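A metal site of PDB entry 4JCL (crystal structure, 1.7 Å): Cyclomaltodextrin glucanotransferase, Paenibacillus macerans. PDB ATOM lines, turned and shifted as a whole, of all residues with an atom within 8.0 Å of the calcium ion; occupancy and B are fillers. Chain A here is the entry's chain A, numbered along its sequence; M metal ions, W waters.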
ATOM      1  N   PRO A 138     -31.795   0.996  -4.654  1.00  0.00           N
ATOM      2  CA  PRO A 138     -30.866   0.472  -5.652  1.00  0.00           C
ATOM      3  C   PRO A 138     -29.565  -0.070  -5.033  1.00  0.00           C
ATOM      4  O   PRO A 138     -28.623  -0.388  -5.750  1.00  0.00           O
ATOM      5  CB  PRO A 138     -30.568   1.701  -6.516  1.00  0.00           C
ATOM      6  CG  PRO A 138     -30.667   2.851  -5.559  1.00  0.00           C
ATOM      7  CD  PRO A 138     -31.749   2.472  -4.578  1.00  0.00           C
ATOM      8  N   ASN A 139     -29.509  -0.174  -3.700  1.00  0.00           N
ATOM      9  CA  ASN A 139     -28.335  -0.737  -3.069  1.00  0.00           C
ATOM     10  C   ASN A 139     -28.189  -2.238  -3.276  1.00  0.00           C
ATOM     11  O   ASN A 139     -27.074  -2.787  -3.288  1.00  0.00           O
ATOM     12  CB  ASN A 139     -28.364  -0.450  -1.564  1.00  0.00           C
ATOM     13  CG  ASN A 139     -27.177  -1.059  -0.853  1.00  0.00           C
ATOM     14  OD1 ASN A 139     -26.051  -0.638  -1.078  1.00  0.00           O
ATOM     15  ND2 ASN A 139     -27.422  -2.064  -0.014  1.00  0.00           N
ATOM     16  N   HIS A 140     -29.311  -2.920  -3.427  1.00  0.00           N
ATOM     17  CA  HIS A 140     -29.313  -4.366  -3.362  1.00  0.00           C
ATOM     18  C   HIS A 140     -30.556  -4.908  -4.033  1.00  0.00           C
ATOM     19  O   HIS A 140     -31.479  -4.159  -4.356  1.00  0.00           O
ATOM     20  CB  HIS A 140     -29.309  -4.806  -1.901  1.00  0.00           C
ATOM     21  CG  HIS A 140     -30.413  -4.169  -1.105  1.00  0.00           C
ATOM     22  ND1 HIS A 140     -30.198  -3.092  -0.262  1.00  0.00           N
ATOM     23  CD2 HIS A 140     -31.736  -4.436  -1.049  1.00  0.00           C
ATOM     24  CE1 HIS A 140     -31.348  -2.728   0.285  1.00  0.00           C
ATOM     25  NE2 HIS A 140     -32.299  -3.538  -0.176  1.00  0.00           N
ATOM     26  N   HIS A 176     -21.337  -7.315  -5.463  1.00  0.00           N
ATOM     27  CA  HIS A 176     -20.145  -7.473  -4.625  1.00  0.00           C
ATOM     28  C   HIS A 176     -20.078  -8.860  -3.968  1.00  0.00           C
ATOM     29  O   HIS A 176     -21.097  -9.377  -3.506  1.00  0.00           O
ATOM     30  CB  HIS A 176     -20.105  -6.394  -3.538  1.00  0.00           C
ATOM     31  CG  HIS A 176     -19.825  -5.022  -4.067  1.00  0.00           C
ATOM     32  ND1 HIS A 176     -20.535  -3.913  -3.652  1.00  0.00           N
ATOM     33  CD2 HIS A 176     -18.909  -4.570  -4.955  1.00  0.00           C
ATOM     34  CE1 HIS A 176     -20.082  -2.843  -4.285  1.00  0.00           C
ATOM     35  NE2 HIS A 176     -19.085  -3.216  -5.072  1.00  0.00           N
ATOM     36  N   GLU A 187     -16.853   2.589   4.902  1.00  0.00           N
ATOM     37  CA  GLU A 187     -16.378   1.807   3.779  1.00  0.00           C
ATOM     38  C   GLU A 187     -16.938   0.403   3.878  1.00  0.00           C
ATOM     39  O   GLU A 187     -17.430  -0.155   2.904  1.00  0.00           O
ATOM     40  CB  GLU A 187     -14.851   1.728   3.778  1.00  0.00           C
ATOM     41  CG  GLU A 187     -14.307   0.725   2.760  1.00  0.00           C
ATOM     42  CD  GLU A 187     -12.799   0.540   2.875  1.00  0.00           C
ATOM     43  OE1 GLU A 187     -12.204   1.050   3.832  1.00  0.00           O
ATOM     44  OE2 GLU A 187     -12.212  -0.110   1.980  1.00  0.00           O
ATOM     45  N   ASP A 188     -16.851  -0.174   5.073  1.00  0.00           N
ATOM     46  CA  ASP A 188     -17.281  -1.553   5.258  1.00  0.00           C
ATOM     47  C   ASP A 188     -18.747  -1.721   4.871  1.00  0.00           C
ATOM     48  O   ASP A 188     -19.145  -2.740   4.298  1.00  0.00           O
ATOM     49  CB  ASP A 188     -17.057  -1.987   6.714  1.00  0.00           C
ATOM     50  CG  ASP A 188     -17.059  -3.496   6.864  1.00  0.00           C
ATOM     51  OD1 ASP A 188     -15.969  -4.105   6.836  1.00  0.00           O
ATOM     52  OD2 ASP A 188     -18.164  -4.068   6.986  1.00  0.00           O
ATOM     53  N   GLY A 189     -19.547  -0.702   5.202  1.00  0.00           N
ATOM     54  CA  GLY A 189     -20.980  -0.750   4.971  1.00  0.00           C
ATOM     55  C   GLY A 189     -21.397  -0.462   3.538  1.00  0.00           C
ATOM     56  O   GLY A 189     -22.538  -0.712   3.152  1.00  0.00           O
ATOM     57  N   ILE A 190     -20.475   0.090   2.750  1.00  0.00           N
ATOM     58  CA  ILE A 190     -20.767   0.410   1.357  1.00  0.00           C
ATOM     59  C   ILE A 190     -20.432  -0.734   0.410  1.00  0.00           C
ATOM     60  O   ILE A 190     -21.201  -1.036  -0.485  1.00  0.00           O
ATOM     61  CB  ILE A 190     -20.034   1.683   0.901  1.00  0.00           C
ATOM     62  CG1 ILE A 190     -20.591   2.918   1.599  1.00  0.00           C
ATOM     63  CG2 ILE A 190     -20.171   1.870  -0.620  1.00  0.00           C
ATOM     64  CD1 ILE A 190     -19.790   4.191   1.322  1.00  0.00           C
ATOM     65  N   TYR A 191     -19.284  -1.377   0.607  1.00  0.00           N
ATOM     66  CA  TYR A 191     -18.798  -2.358  -0.363  1.00  0.00           C
ATOM     67  C   TYR A 191     -18.950  -3.829   0.047  1.00  0.00           C
ATOM     68  O   TYR A 191     -18.460  -4.733  -0.621  1.00  0.00           O
ATOM     69  CB  TYR A 191     -17.360  -2.028  -0.778  1.00  0.00           C
ATOM     70  CG  TYR A 191     -17.290  -0.686  -1.478  1.00  0.00           C
ATOM     71  CD1 TYR A 191     -17.699  -0.547  -2.792  1.00  0.00           C
ATOM     72  CD2 TYR A 191     -16.843   0.441  -0.804  1.00  0.00           C
ATOM     73  CE1 TYR A 191     -17.663   0.686  -3.438  1.00  0.00           C
ATOM     74  CE2 TYR A 191     -16.790   1.673  -1.434  1.00  0.00           C
ATOM     75  CZ  TYR A 191     -17.200   1.787  -2.749  1.00  0.00           C
ATOM     76  OH  TYR A 191     -17.147   3.019  -3.379  1.00  0.00           O
ATOM     77  N   LYS A 192     -19.677  -4.056   1.128  1.00  0.00           N
ATOM     78  CA  LYS A 192     -20.083  -5.398   1.531  1.00  0.00           C
ATOM     79  C   LYS A 192     -21.597  -5.456   1.616  1.00  0.00           C
ATOM     80  O   LYS A 192     -22.275  -4.431   1.545  1.00  0.00           O
ATOM     81  CB  LYS A 192     -19.482  -5.726   2.893  1.00  0.00           C
ATOM     82  CG  LYS A 192     -17.972  -5.703   2.906  1.00  0.00           C
ATOM     83  CD  LYS A 192     -17.437  -6.208   4.231  1.00  0.00           C
ATOM     84  CE  LYS A 192     -15.930  -6.209   4.227  1.00  0.00           C
ATOM     85  NZ  LYS A 192     -15.391  -6.844   5.474  1.00  0.00           N
ATOM     86  N   ASN A 193     -22.145  -6.648   1.781  1.00  0.00           N
ATOM     87  CA  ASN A 193     -23.594  -6.783   1.759  1.00  0.00           C
ATOM     88  C   ASN A 193     -24.225  -6.190   3.012  1.00  0.00           C
ATOM     89  O   ASN A 193     -23.740  -6.393   4.114  1.00  0.00           O
ATOM     90  CB  ASN A 193     -24.004  -8.253   1.674  1.00  0.00           C
ATOM     91  CG  ASN A 193     -23.572  -8.902   0.371  1.00  0.00           C
ATOM     92  OD1 ASN A 193     -23.366  -8.221  -0.632  1.00  0.00           O
ATOM     93  ND2 ASN A 193     -23.419 -10.222   0.393  1.00  0.00           N
ATOM     94  N   LEU A 194     -25.342  -5.483   2.824  1.00  0.00           N
ATOM     95  CA  LEU A 194     -26.155  -5.026   3.930  1.00  0.00           C
ATOM     96  C   LEU A 194     -26.938  -6.240   4.433  1.00  0.00           C
ATOM     97  O   LEU A 194     -27.813  -6.758   3.731  1.00  0.00           O
ATOM     98  CB  LEU A 194     -27.094  -3.919   3.441  1.00  0.00           C
ATOM     99  CG  LEU A 194     -28.026  -3.229   4.429  1.00  0.00           C
ATOM    100  CD1 LEU A 194     -27.245  -2.550   5.556  1.00  0.00           C
ATOM    101  CD2 LEU A 194     -28.908  -2.219   3.688  1.00  0.00           C
ATOM    102  N   LEU A 197     -28.224  -9.069   1.983  1.00  0.00           N
ATOM    103  CA  LEU A 197     -28.817  -8.583   0.728  1.00  0.00           C
ATOM    104  C   LEU A 197     -27.738  -8.480  -0.350  1.00  0.00           C
ATOM    105  O   LEU A 197     -26.711  -7.845  -0.138  1.00  0.00           O
ATOM    106  CB  LEU A 197     -29.494  -7.223   0.930  1.00  0.00           C
ATOM    107  CG  LEU A 197     -30.575  -7.216   2.027  1.00  0.00           C
ATOM    108  CD1 LEU A 197     -30.917  -5.807   2.491  1.00  0.00           C
ATOM    109  CD2 LEU A 197     -31.830  -7.947   1.553  1.00  0.00           C
ATOM    110  N   ALA A 198     -27.971  -9.121  -1.485  1.00  0.00           N
ATOM    111  CA  ALA A 198     -26.972  -9.118  -2.551  1.00  0.00           C
ATOM    112  C   ALA A 198     -26.662  -7.683  -2.949  1.00  0.00           C
ATOM    113  O   ALA A 198     -27.525  -6.963  -3.430  1.00  0.00           O
ATOM    114  CB  ALA A 198     -27.445  -9.939  -3.764  1.00  0.00           C
ATOM    115  N   ASP A 199     -25.414  -7.267  -2.740  1.00  0.00           N
ATOM    116  CA  ASP A 199     -25.040  -5.862  -2.919  1.00  0.00           C
ATOM    117  C   ASP A 199     -24.697  -5.542  -4.365  1.00  0.00           C
ATOM    118  O   ASP A 199     -23.783  -6.136  -4.938  1.00  0.00           O
ATOM    119  CB  ASP A 199     -23.832  -5.547  -2.034  1.00  0.00           C
ATOM    120  CG  ASP A 199     -23.748  -4.088  -1.665  1.00  0.00           C
ATOM    121  OD1 ASP A 199     -24.734  -3.582  -1.080  1.00  0.00           O
ATOM    122  OD2 ASP A 199     -22.712  -3.459  -1.976  1.00  0.00           O
ATOM    123  N   ILE A 200     -25.437  -4.595  -4.953  1.00  0.00           N
ATOM    124  CA  ILE A 200     -25.195  -4.119  -6.312  1.00  0.00           C
ATOM    125  C   ILE A 200     -23.820  -3.456  -6.459  1.00  0.00           C
ATOM    126  O   ILE A 200     -23.392  -2.682  -5.603  1.00  0.00           O
ATOM    127  CB  ILE A 200     -26.282  -3.111  -6.765  1.00  0.00           C
ATOM    128  CG1 ILE A 200     -27.651  -3.787  -6.838  1.00  0.00           C
ATOM    129  CG2 ILE A 200     -25.912  -2.479  -8.099  1.00  0.00           C
ATOM    130  CD1 ILE A 200     -27.748  -4.848  -7.925  1.00  0.00           C
ATOM    131  N   ASN A 201     -23.145  -3.754  -7.561  1.00  0.00           N
ATOM    132  CA  ASN A 201     -21.876  -3.135  -7.890  1.00  0.00           C
ATOM    133  C   ASN A 201     -22.095  -2.038  -8.913  1.00  0.00           C
ATOM    134  O   ASN A 201     -22.176  -2.310 -10.116  1.00  0.00           O
ATOM    135  CB  ASN A 201     -20.916  -4.204  -8.447  1.00  0.00           C
ATOM    136  CG  ASN A 201     -19.692  -3.596  -9.079  1.00  0.00           C
ATOM    137  OD1 ASN A 201     -19.404  -2.419  -8.864  1.00  0.00           O
ATOM    138  ND2 ASN A 201     -18.969  -4.390  -9.863  1.00  0.00           N
ATOM    139  N   HIS A 202     -22.199  -0.791  -8.447  1.00  0.00           N
ATOM    140  CA  HIS A 202     -22.568   0.313  -9.338  1.00  0.00           C
ATOM    141  C   HIS A 202     -21.399   0.778 -10.193  1.00  0.00           C
ATOM    142  O   HIS A 202     -21.567   1.627 -11.068  1.00  0.00           O
ATOM    143  CB  HIS A 202     -23.123   1.502  -8.542  1.00  0.00           C
ATOM    144  CG  HIS A 202     -24.336   1.162  -7.733  1.00  0.00           C
ATOM    145  ND1 HIS A 202     -24.257   0.702  -6.442  1.00  0.00           N
ATOM    146  CD2 HIS A 202     -25.648   1.177  -8.050  1.00  0.00           C
ATOM    147  CE1 HIS A 202     -25.475   0.455  -5.984  1.00  0.00           C
ATOM    148  NE2 HIS A 202     -26.341   0.749  -6.936  1.00  0.00           N
ATOM    149  N   ALA A 230     -31.100   3.377   2.324  1.00  0.00           N
ATOM    150  CA  ALA A 230     -29.740   2.935   2.659  1.00  0.00           C
ATOM    151  C   ALA A 230     -28.650   3.764   1.980  1.00  0.00           C
ATOM    152  O   ALA A 230     -27.699   3.206   1.421  1.00  0.00           O
ATOM    153  CB  ALA A 230     -29.566   1.453   2.305  1.00  0.00           C
ATOM    154  N   VAL A 231     -28.783   5.090   2.015  1.00  0.00           N
ATOM    155  CA  VAL A 231     -27.825   5.939   1.292  1.00  0.00           C
ATOM    156  C   VAL A 231     -26.416   5.868   1.877  1.00  0.00           C
ATOM    157  O   VAL A 231     -25.455   6.153   1.197  1.00  0.00           O
ATOM    158  CB  VAL A 231     -28.301   7.412   1.207  1.00  0.00           C
ATOM    159  CG1 VAL A 231     -29.634   7.478   0.462  1.00  0.00           C
ATOM    160  CG2 VAL A 231     -28.425   8.034   2.605  1.00  0.00           C
ATOM    161  N   LYS A 232     -26.311   5.465   3.137  1.00  0.00           N
ATOM    162  CA  LYS A 232     -25.003   5.335   3.784  1.00  0.00           C
ATOM    163  C   LYS A 232     -24.259   4.133   3.236  1.00  0.00           C
ATOM    164  O   LYS A 232     -23.059   3.950   3.476  1.00  0.00           O
ATOM    165  CB  LYS A 232     -25.185   5.186   5.298  1.00  0.00           C
ATOM    166  CG  LYS A 232     -23.924   5.259   6.134  1.00  0.00           C
ATOM    167  CD  LYS A 232     -24.301   5.127   7.616  1.00  0.00           C
ATOM    168  CE  LYS A 232     -23.097   5.131   8.537  1.00  0.00           C
ATOM    169  NZ  LYS A 232     -23.535   4.835   9.947  1.00  0.00           N
ATOM    170  N   HIS A 233     -24.977   3.301   2.484  1.00  0.00           N
ATOM    171  CA  HIS A 233     -24.464   2.006   2.063  1.00  0.00           C
ATOM    172  C   HIS A 233     -24.134   1.943   0.583  1.00  0.00           C
ATOM    173  O   HIS A 233     -23.721   0.904   0.094  1.00  0.00           O
ATOM    174  CB  HIS A 233     -25.431   0.908   2.481  1.00  0.00           C
ATOM    175  CG  HIS A 233     -25.586   0.815   3.964  1.00  0.00           C
ATOM    176  ND1 HIS A 233     -24.623   0.223   4.768  1.00  0.00           N
ATOM    177  CD2 HIS A 233     -26.525   1.304   4.806  1.00  0.00           C
ATOM    178  CE1 HIS A 233     -24.988   0.323   6.031  1.00  0.00           C
ATOM    179  NE2 HIS A 233     -26.132   0.982   6.084  1.00  0.00           N
ATOM    180  N   MET A 234     -24.304   3.067  -0.108  1.00  0.00           N
ATOM    181  CA  MET A 234     -23.905   3.189  -1.511  1.00  0.00           C
ATOM    182  C   MET A 234     -22.834   4.263  -1.604  1.00  0.00           C
ATOM    183  O   MET A 234     -22.750   5.115  -0.722  1.00  0.00           O
ATOM    184  CB  MET A 234     -25.103   3.556  -2.398  1.00  0.00           C
ATOM    185  CG  MET A 234     -26.130   2.401  -2.543  1.00  0.00           C
ATOM    186  SD  MET A 234     -27.608   2.890  -3.423  1.00  0.00           S
ATOM    187  CE  MET A 234     -28.430   3.955  -2.213  1.00  0.00           C
ATOM    188  N   PRO A 235     -22.026   4.243  -2.662  1.00  0.00           N
ATOM    189  CA  PRO A 235     -20.993   5.282  -2.769  1.00  0.00           C
ATOM    190  C   PRO A 235     -21.608   6.669  -2.939  1.00  0.00           C
ATOM    191  O   PRO A 235     -22.519   6.856  -3.754  1.00  0.00           O
ATOM    192  CB  PRO A 235     -20.223   4.893  -4.032  1.00  0.00           C
ATOM    193  CG  PRO A 235     -20.517   3.421  -4.234  1.00  0.00           C
ATOM    194  CD  PRO A 235     -21.944   3.254  -3.754  1.00  0.00           C
HETATM  195 CA    CA M   1     -23.698  -1.225  -1.143  1.00  0.00          CA
HETATM  196  O   HOH W   1     -24.657  -1.487  -3.487  1.00  0.00           O
HETATM  197  O   HOH W   2     -22.211   0.082  -2.709  1.00  0.00           O
HETATM  198  O   HOH W   3     -23.822  -2.032   1.237  1.00  0.00           O
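The backbone NH of Asn 139 lies within hydrogen-bond range of the side-chain sulfur of Met 234 (3.6 Å).
The backbone carbonyl oxygen (O) of Asn 139 lies within hydrogen-bond range of the backbone NH (N) of Ile 200 (3.0 Å).
A ring nitrogen (ND1) of His 140 lies within hydrogen-bond range of the side-chain amide nitrogen (ND2) of Asn 139 (3.0 Å).
The backbone carbonyl oxygen (O) of Gly 189 lies within hydrogen-bond range of a ring nitrogen (ND1) of His 233, 2.8 Å away.
O of Asp 199 sits at hydrogen-bond distance from N of His 176, at 2.8 Å.
The side-chain amide oxygen of Asn 193 lies close to the backbone NH of Asp 199 (3.1 Å).
Water W1 bridges the backbone carbonyl oxygen of Ile 200 and the backbone carbonyl oxygen of Asn 139.
The calcium ion is bound by the side-chain amide oxygen (OD1) of Asn 139, the backbone carbonyl oxygen (O) of His 233, water W3, water W2, water W1, the side-chain carboxylate (OD1) of Asp 199, the side-chain carboxylate (OD2) of Asp 199 and the backbone carbonyl oxygen (O) of Ile 190.
The calcium ion has eight donor atoms within binding distance.
The nearest printed residue that does not touch the calcium ion is Lys 192 (4.4 Å).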
